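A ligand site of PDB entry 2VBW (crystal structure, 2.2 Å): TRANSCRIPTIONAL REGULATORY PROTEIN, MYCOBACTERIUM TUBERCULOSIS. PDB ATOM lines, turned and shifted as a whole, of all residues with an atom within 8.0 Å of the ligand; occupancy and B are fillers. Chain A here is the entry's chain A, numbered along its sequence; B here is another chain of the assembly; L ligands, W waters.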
ATOM      1  N   ILE A  73     -22.408  -8.952 -18.610  1.00  0.00           N
ATOM      2  CA  ILE A  73     -21.403  -9.697 -17.847  1.00  0.00           C
ATOM      3  C   ILE A  73     -20.258 -10.163 -18.741  1.00  0.00           C
ATOM      4  O   ILE A  73     -20.438 -10.457 -19.917  1.00  0.00           O
ATOM      5  CB  ILE A  73     -21.994 -10.887 -16.986  1.00  0.00           C
ATOM      6  CG1 ILE A  73     -22.687 -11.928 -17.869  1.00  0.00           C
ATOM      7  CG2 ILE A  73     -22.966 -10.422 -15.956  1.00  0.00           C
ATOM      8  CD1 ILE A  73     -23.130 -13.188 -17.156  1.00  0.00           C
ATOM      9  N   THR A  74     -19.070 -10.183 -18.170  1.00  0.00           N
ATOM     10  CA  THR A  74     -17.911 -10.717 -18.805  1.00  0.00           C
ATOM     11  C   THR A  74     -17.034 -11.614 -17.847  1.00  0.00           C
ATOM     12  O   THR A  74     -16.778 -11.264 -16.705  1.00  0.00           O
ATOM     13  CB  THR A  74     -17.185  -9.696 -19.749  1.00  0.00           C
ATOM     14  OG1 THR A  74     -15.797  -9.708 -19.505  1.00  0.00           O
ATOM     15  CG2 THR A  74     -17.644  -8.328 -19.640  1.00  0.00           C
ATOM     16  N   PRO A  75     -16.621 -12.814 -18.322  1.00  0.00           N
ATOM     17  CA  PRO A  75     -15.840 -13.756 -17.466  1.00  0.00           C
ATOM     18  C   PRO A  75     -14.662 -13.094 -16.814  1.00  0.00           C
ATOM     19  O   PRO A  75     -13.973 -12.322 -17.463  1.00  0.00           O
ATOM     20  CB  PRO A  75     -15.366 -14.802 -18.461  1.00  0.00           C
ATOM     21  CG  PRO A  75     -16.570 -14.845 -19.450  1.00  0.00           C
ATOM     22  CD  PRO A  75     -16.860 -13.392 -19.676  1.00  0.00           C
ATOM     23  N   PRO A  78     -11.444 -15.688 -18.949  1.00  0.00           N
ATOM     24  CA  PRO A  78     -11.980 -16.186 -20.229  1.00  0.00           C
ATOM     25  C   PRO A  78     -11.472 -17.555 -20.677  1.00  0.00           C
ATOM     26  O   PRO A  78     -12.037 -18.105 -21.622  1.00  0.00           O
ATOM     27  CB  PRO A  78     -11.605 -15.101 -21.229  1.00  0.00           C
ATOM     28  CG  PRO A  78     -10.428 -14.365 -20.597  1.00  0.00           C
ATOM     29  CD  PRO A  78     -10.561 -14.519 -19.111  1.00  0.00           C
ATOM     30  N   ASP A  82     -17.029 -21.877 -20.726  1.00  0.00           N
ATOM     31  CA  ASP A  82     -18.087 -20.871 -20.747  1.00  0.00           C
ATOM     32  C   ASP A  82     -19.543 -21.341 -20.598  1.00  0.00           C
ATOM     33  O   ASP A  82     -20.242 -21.605 -21.575  1.00  0.00           O
ATOM     34  CB  ASP A  82     -17.946 -19.860 -21.877  1.00  0.00           C
ATOM     35  CG  ASP A  82     -18.900 -18.681 -21.692  1.00  0.00           C
ATOM     36  OD1 ASP A  82     -19.259 -18.303 -20.535  1.00  0.00           O
ATOM     37  OD2 ASP A  82     -19.312 -18.149 -22.732  1.00  0.00           O
ATOM     38  N   ASP A  83     -19.951 -21.379 -19.332  1.00  0.00           N
ATOM     39  CA  ASP A  83     -21.240 -21.855 -18.928  1.00  0.00           C
ATOM     40  C   ASP A  83     -21.992 -20.852 -18.022  1.00  0.00           C
ATOM     41  O   ASP A  83     -22.731 -21.254 -17.127  1.00  0.00           O
ATOM     42  CB  ASP A  83     -21.064 -23.198 -18.208  1.00  0.00           C
ATOM     43  CG  ASP A  83     -20.086 -23.109 -17.039  1.00  0.00           C
ATOM     44  OD1 ASP A  83     -19.377 -22.073 -16.886  1.00  0.00           O
ATOM     45  OD2 ASP A  83     -20.024 -24.109 -16.263  1.00  0.00           O
ATOM     46  N   ALA A  84     -21.829 -19.550 -18.254  1.00  0.00           N
ATOM     47  CA  ALA A  84     -22.535 -18.541 -17.436  1.00  0.00           C
ATOM     48  C   ALA A  84     -24.058 -18.722 -17.476  1.00  0.00           C
ATOM     49  O   ALA A  84     -24.673 -18.720 -16.452  1.00  0.00           O
ATOM     50  CB  ALA A  84     -22.097 -17.088 -17.760  1.00  0.00           C
ATOM     51  N   PRO A  85     -24.656 -18.879 -18.664  1.00  0.00           N
ATOM     52  CA  PRO A  85     -26.123 -19.025 -18.715  1.00  0.00           C
ATOM     53  C   PRO A  85     -26.739 -20.149 -17.870  1.00  0.00           C
ATOM     54  O   PRO A  85     -27.783 -19.949 -17.211  1.00  0.00           O
ATOM     55  CB  PRO A  85     -26.397 -19.296 -20.201  1.00  0.00           C
ATOM     56  CG  PRO A  85     -25.169 -18.819 -20.921  1.00  0.00           C
ATOM     57  CD  PRO A  85     -24.043 -18.869 -19.995  1.00  0.00           C
ATOM     58  N   TYR A  98     -28.928 -13.263 -22.898  1.00  0.00           N
ATOM     59  CA  TYR A  98     -28.541 -13.275 -24.302  1.00  0.00           C
ATOM     60  C   TYR A  98     -27.027 -13.247 -24.396  1.00  0.00           C
ATOM     61  O   TYR A  98     -26.384 -12.597 -23.580  1.00  0.00           O
ATOM     62  CB  TYR A  98     -29.024 -11.988 -24.986  1.00  0.00           C
ATOM     63  CG  TYR A  98     -30.471 -11.681 -24.801  1.00  0.00           C
ATOM     64  CD1 TYR A  98     -30.914 -10.880 -23.760  1.00  0.00           C
ATOM     65  CD2 TYR A  98     -31.424 -12.174 -25.721  1.00  0.00           C
ATOM     66  CE1 TYR A  98     -32.274 -10.606 -23.561  1.00  0.00           C
ATOM     67  CE2 TYR A  98     -32.776 -11.917 -25.558  1.00  0.00           C
ATOM     68  CZ  TYR A  98     -33.203 -11.132 -24.482  1.00  0.00           C
ATOM     69  OH  TYR A  98     -34.572 -10.878 -24.358  1.00  0.00           O
ATOM     70  N   SER A  99     -26.435 -13.898 -25.414  1.00  0.00           N
ATOM     71  CA  SER A  99     -25.045 -13.693 -25.718  1.00  0.00           C
ATOM     72  C   SER A  99     -25.019 -12.602 -26.802  1.00  0.00           C
ATOM     73  O   SER A  99     -25.948 -12.459 -27.628  1.00  0.00           O
ATOM     74  CB  SER A  99     -24.351 -14.965 -26.160  1.00  0.00           C
ATOM     75  OG  SER A  99     -25.030 -15.487 -27.281  1.00  0.00           O
ATOM     76  N   VAL A 100     -23.953 -11.836 -26.804  1.00  0.00           N
ATOM     77  CA  VAL A 100     -23.947 -10.569 -27.518  1.00  0.00           C
ATOM     78  C   VAL A 100     -22.588 -10.408 -28.211  1.00  0.00           C
ATOM     79  O   VAL A 100     -21.576 -10.929 -27.750  1.00  0.00           O
ATOM     80  CB  VAL A 100     -24.367  -9.531 -26.439  1.00  0.00           C
ATOM     81  CG1 VAL A 100     -23.306  -8.640 -25.860  1.00  0.00           C
ATOM     82  CG2 VAL A 100     -25.904  -9.161 -26.401  1.00  0.00           C
ATOM     83  N   ALA A 101     -22.566  -9.726 -29.352  1.00  0.00           N
ATOM     84  CA  ALA A 101     -21.314  -9.333 -30.008  1.00  0.00           C
ATOM     85  C   ALA A 101     -20.725  -8.109 -29.323  1.00  0.00           C
ATOM     86  O   ALA A 101     -21.458  -7.258 -28.885  1.00  0.00           O
ATOM     87  CB  ALA A 101     -21.561  -9.084 -31.442  1.00  0.00           C
ATOM     88  N   GLY A 102     -19.409  -8.021 -29.219  1.00  0.00           N
ATOM     89  CA  GLY A 102     -18.773  -6.891 -28.568  1.00  0.00           C
ATOM     90  C   GLY A 102     -17.836  -7.318 -27.453  1.00  0.00           C
ATOM     91  O   GLY A 102     -17.385  -8.440 -27.419  1.00  0.00           O
ATOM     92  N   GLU A 103     -17.570  -6.411 -26.522  1.00  0.00           N
ATOM     93  CA  GLU A 103     -16.606  -6.624 -25.442  1.00  0.00           C
ATOM     94  C   GLU A 103     -17.185  -7.503 -24.334  1.00  0.00           C
ATOM     95  O   GLU A 103     -16.573  -8.442 -23.864  1.00  0.00           O
ATOM     96  CB  GLU A 103     -16.286  -5.248 -24.872  1.00  0.00           C
ATOM     97  CG  GLU A 103     -14.888  -5.221 -24.249  1.00  0.00           C
ATOM     98  CD  GLU A 103     -14.544  -3.811 -23.650  1.00  0.00           C
ATOM     99  OE1 GLU A 103     -14.071  -3.779 -22.470  1.00  0.00           O
ATOM    100  OE2 GLU A 103     -14.795  -2.759 -24.328  1.00  0.00           O
ATOM    101  N   GLU A 104     -18.422  -7.275 -23.996  1.00  0.00           N
ATOM    102  CA  GLU A 104     -19.146  -8.149 -23.084  1.00  0.00           C
ATOM    103  C   GLU A 104     -19.629  -9.438 -23.764  1.00  0.00           C
ATOM    104  O   GLU A 104     -19.691  -9.505 -25.006  1.00  0.00           O
ATOM    105  CB  GLU A 104     -20.280  -7.353 -22.457  1.00  0.00           C
ATOM    106  CG  GLU A 104     -19.557  -6.347 -21.503  1.00  0.00           C
ATOM    107  CD  GLU A 104     -20.146  -4.950 -21.477  1.00  0.00           C
ATOM    108  OE1 GLU A 104     -20.938  -4.568 -22.394  1.00  0.00           O
ATOM    109  OE2 GLU A 104     -19.782  -4.241 -20.530  1.00  0.00           O
ATOM    110  N   SER A 105     -19.912 -10.450 -22.937  1.00  0.00           N
ATOM    111  CA  SER A 105     -20.347 -11.770 -23.364  1.00  0.00           C
ATOM    112  C   SER A 105     -21.841 -11.979 -23.304  1.00  0.00           C
ATOM    113  O   SER A 105     -22.395 -12.510 -24.252  1.00  0.00           O
ATOM    114  CB  SER A 105     -19.645 -12.873 -22.523  1.00  0.00           C
ATOM    115  OG  SER A 105     -18.256 -12.700 -22.586  1.00  0.00           O
ATOM    116  N   TYR A 106     -22.490 -11.541 -22.238  1.00  0.00           N
ATOM    117  CA  TYR A 106     -23.892 -11.811 -22.045  1.00  0.00           C
ATOM    118  C   TYR A 106     -24.496 -10.551 -21.521  1.00  0.00           C
ATOM    119  O   TYR A 106     -23.843  -9.765 -20.824  1.00  0.00           O
ATOM    120  CB  TYR A 106     -24.189 -12.998 -21.041  1.00  0.00           C
ATOM    121  CG  TYR A 106     -23.496 -14.278 -21.420  1.00  0.00           C
ATOM    122  CD1 TYR A 106     -24.059 -15.131 -22.387  1.00  0.00           C
ATOM    123  CD2 TYR A 106     -22.209 -14.598 -20.909  1.00  0.00           C
ATOM    124  CE1 TYR A 106     -23.435 -16.267 -22.793  1.00  0.00           C
ATOM    125  CE2 TYR A 106     -21.547 -15.770 -21.315  1.00  0.00           C
ATOM    126  CZ  TYR A 106     -22.192 -16.583 -22.273  1.00  0.00           C
ATOM    127  OH  TYR A 106     -21.657 -17.747 -22.758  1.00  0.00           O
ATOM    128  N   VAL A 107     -25.767 -10.374 -21.897  1.00  0.00           N
ATOM    129  CA  VAL A 107     -26.608  -9.342 -21.342  1.00  0.00           C
ATOM    130  C   VAL A 107     -27.773 -10.072 -20.617  1.00  0.00           C
ATOM    131  O   VAL A 107     -28.399 -10.938 -21.198  1.00  0.00           O
ATOM    132  CB  VAL A 107     -27.148  -8.407 -22.457  1.00  0.00           C
ATOM    133  CG1 VAL A 107     -28.319  -7.609 -21.956  1.00  0.00           C
ATOM    134  CG2 VAL A 107     -26.029  -7.471 -23.005  1.00  0.00           C
ATOM    135  N   ILE B 137     -25.581  -6.381 -31.205  1.00  0.00           N
ATOM    136  CA  ILE B 137     -26.193  -7.545 -31.857  1.00  0.00           C
ATOM    137  C   ILE B 137     -26.236  -8.740 -30.887  1.00  0.00           C
ATOM    138  O   ILE B 137     -25.259  -9.069 -30.235  1.00  0.00           O
ATOM    139  CB  ILE B 137     -25.455  -7.874 -33.213  1.00  0.00           C
ATOM    140  CG1 ILE B 137     -25.947  -6.989 -34.378  1.00  0.00           C
ATOM    141  CG2 ILE B 137     -25.842  -9.253 -33.771  1.00  0.00           C
ATOM    142  CD1 ILE B 137     -25.690  -5.592 -34.272  1.00  0.00           C
ATOM    143  N   LEU B 139     -26.458 -12.729 -30.383  1.00  0.00           N
ATOM    144  CA  LEU B 139     -26.012 -13.879 -31.107  1.00  0.00           C
ATOM    145  C   LEU B 139     -26.971 -15.069 -30.864  1.00  0.00           C
ATOM    146  O   LEU B 139     -27.432 -15.753 -31.819  1.00  0.00           O
ATOM    147  CB  LEU B 139     -24.569 -14.245 -30.705  1.00  0.00           C
ATOM    148  CG  LEU B 139     -23.536 -13.179 -31.011  1.00  0.00           C
ATOM    149  CD1 LEU B 139     -22.216 -13.658 -30.408  1.00  0.00           C
ATOM    150  CD2 LEU B 139     -23.441 -12.870 -32.548  1.00  0.00           C
ATOM    151  N   ASN B 140     -27.328 -15.246 -29.594  1.00  0.00           N
ATOM    152  CA  ASN B 140     -28.234 -16.293 -29.176  1.00  0.00           C
ATOM    153  C   ASN B 140     -29.067 -15.847 -27.989  1.00  0.00           C
ATOM    154  O   ASN B 140     -28.616 -15.073 -27.160  1.00  0.00           O
ATOM    155  CB  ASN B 140     -27.445 -17.576 -28.813  1.00  0.00           C
ATOM    156  CG  ASN B 140     -28.352 -18.795 -28.632  1.00  0.00           C
ATOM    157  OD1 ASN B 140     -29.442 -18.889 -29.204  1.00  0.00           O
ATOM    158  ND2 ASN B 140     -27.929 -19.688 -27.792  1.00  0.00           N
ATOM    159  N   PHE B 142     -30.640 -17.448 -24.663  1.00  0.00           N
ATOM    160  CA  PHE B 142     -30.612 -18.679 -23.876  1.00  0.00           C
ATOM    161  C   PHE B 142     -31.908 -18.942 -23.167  1.00  0.00           C
ATOM    162  O   PHE B 142     -32.330 -20.083 -23.118  1.00  0.00           O
ATOM    163  CB  PHE B 142     -29.445 -18.744 -22.882  1.00  0.00           C
ATOM    164  CG  PHE B 142     -28.138 -18.824 -23.552  1.00  0.00           C
ATOM    165  CD1 PHE B 142     -27.517 -17.658 -24.040  1.00  0.00           C
ATOM    166  CD2 PHE B 142     -27.554 -20.076 -23.812  1.00  0.00           C
ATOM    167  CE1 PHE B 142     -26.275 -17.707 -24.729  1.00  0.00           C
ATOM    168  CE2 PHE B 142     -26.316 -20.162 -24.520  1.00  0.00           C
ATOM    169  CZ  PHE B 142     -25.677 -18.961 -24.987  1.00  0.00           C
HETATM  170  N1  LIG L   1     -18.659 -10.995 -27.163  1.00  0.00           N
HETATM  171  C1  LIG L   1     -18.028 -12.026 -28.044  1.00  0.00           C
HETATM  172  C2  LIG L   1     -17.637 -11.425 -29.395  1.00  0.00           C
HETATM  173  O1  LIG L   1     -16.946 -12.071 -30.178  1.00  0.00           O
HETATM  174  C3  LIG L   1     -18.960 -13.259 -28.261  1.00  0.00           C
HETATM  175  C4  LIG L   1     -19.127 -14.136 -27.039  1.00  0.00           C
HETATM  176  C5  LIG L   1     -18.048 -14.914 -26.551  1.00  0.00           C
HETATM  177  C6  LIG L   1     -20.355 -14.208 -26.377  1.00  0.00           C
HETATM  178  C7  LIG L   1     -18.194 -15.744 -25.399  1.00  0.00           C
HETATM  179  C8  LIG L   1     -20.529 -15.001 -25.246  1.00  0.00           C
HETATM  180  C9  LIG L   1     -19.432 -15.802 -24.752  1.00  0.00           C
HETATM  181  O2  LIG L   1     -17.979 -10.256 -29.725  1.00  0.00           O
HETATM  182  O   HOH W   1     -17.051 -11.415 -24.811  1.00  0.00           O
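N1 of the ligand is in hydrogen-bond range of O of Gly 102 (2.9 Å).
A nitrogen (N1) of the ligand lies within hydrogen-bond range of the backbone carbonyl oxygen of Glu 104, 2.8 Å away.
O2 of the ligand is in hydrogen-bond range of N of Gly 102 (2.7 Å).
The backbone carbonyl oxygen of Val 100 sits at hydrogen-bond distance from a nitrogen (N1) of the ligand.
Water W1 lies within hydrogen-bond range of the side-chain hydroxyl of Ser 105 (2.8 Å), a nitrogen (N1) of the ligand (2.9 Å), the backbone carbonyl oxygen of Glu 103 (3.2 Å) and the backbone carbonyl oxygen of Glu 104 (3.3 Å).
N of Ile 73 lies within hydrogen-bond range of O of Tyr 106.
The backbone carbonyl oxygen (O) of Ile 73 lies within hydrogen-bond range of the backbone NH (N) of Ser 105 (3.1 Å).
O of Ser 105 lies within hydrogen-bond range of N of Val 100, 3.1 Å away.
OD1 of Asp 82 sits close to OH of Tyr 106 (3.3 Å).
N of Leu 139 of chain B is in hydrogen-bond range of O of Ser 99.
The backbone NH (N) of Ala 101 sits at hydrogen-bond distance from the backbone carbonyl oxygen (O) of Ile 137 of chain B, 2.9 Å away.
The backbone carbonyl oxygen (O) of Asn 140 of chain B lies within hydrogen-bond range of the backbone NH (N) of Ser 99, 3.0 Å away.
Residues that only touch the ligand: Asp 82, Ser 105, Ala 101, Tyr 106, Leu 139 of chain B and Ser 99.
Hydrophobic or aromatic side chains that line the ligand: Tyr 106 and Leu 139 of chain B.
Within 4 Å of the ligand: Asp 82, Ser 99, Val 100, Ala 101, Gly 102, Glu 104, Ser 105, Tyr 106 and Leu 139 of chain B.
The nearest printed residue that does not touch the ligand is Glu 103 (4.7 Å).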
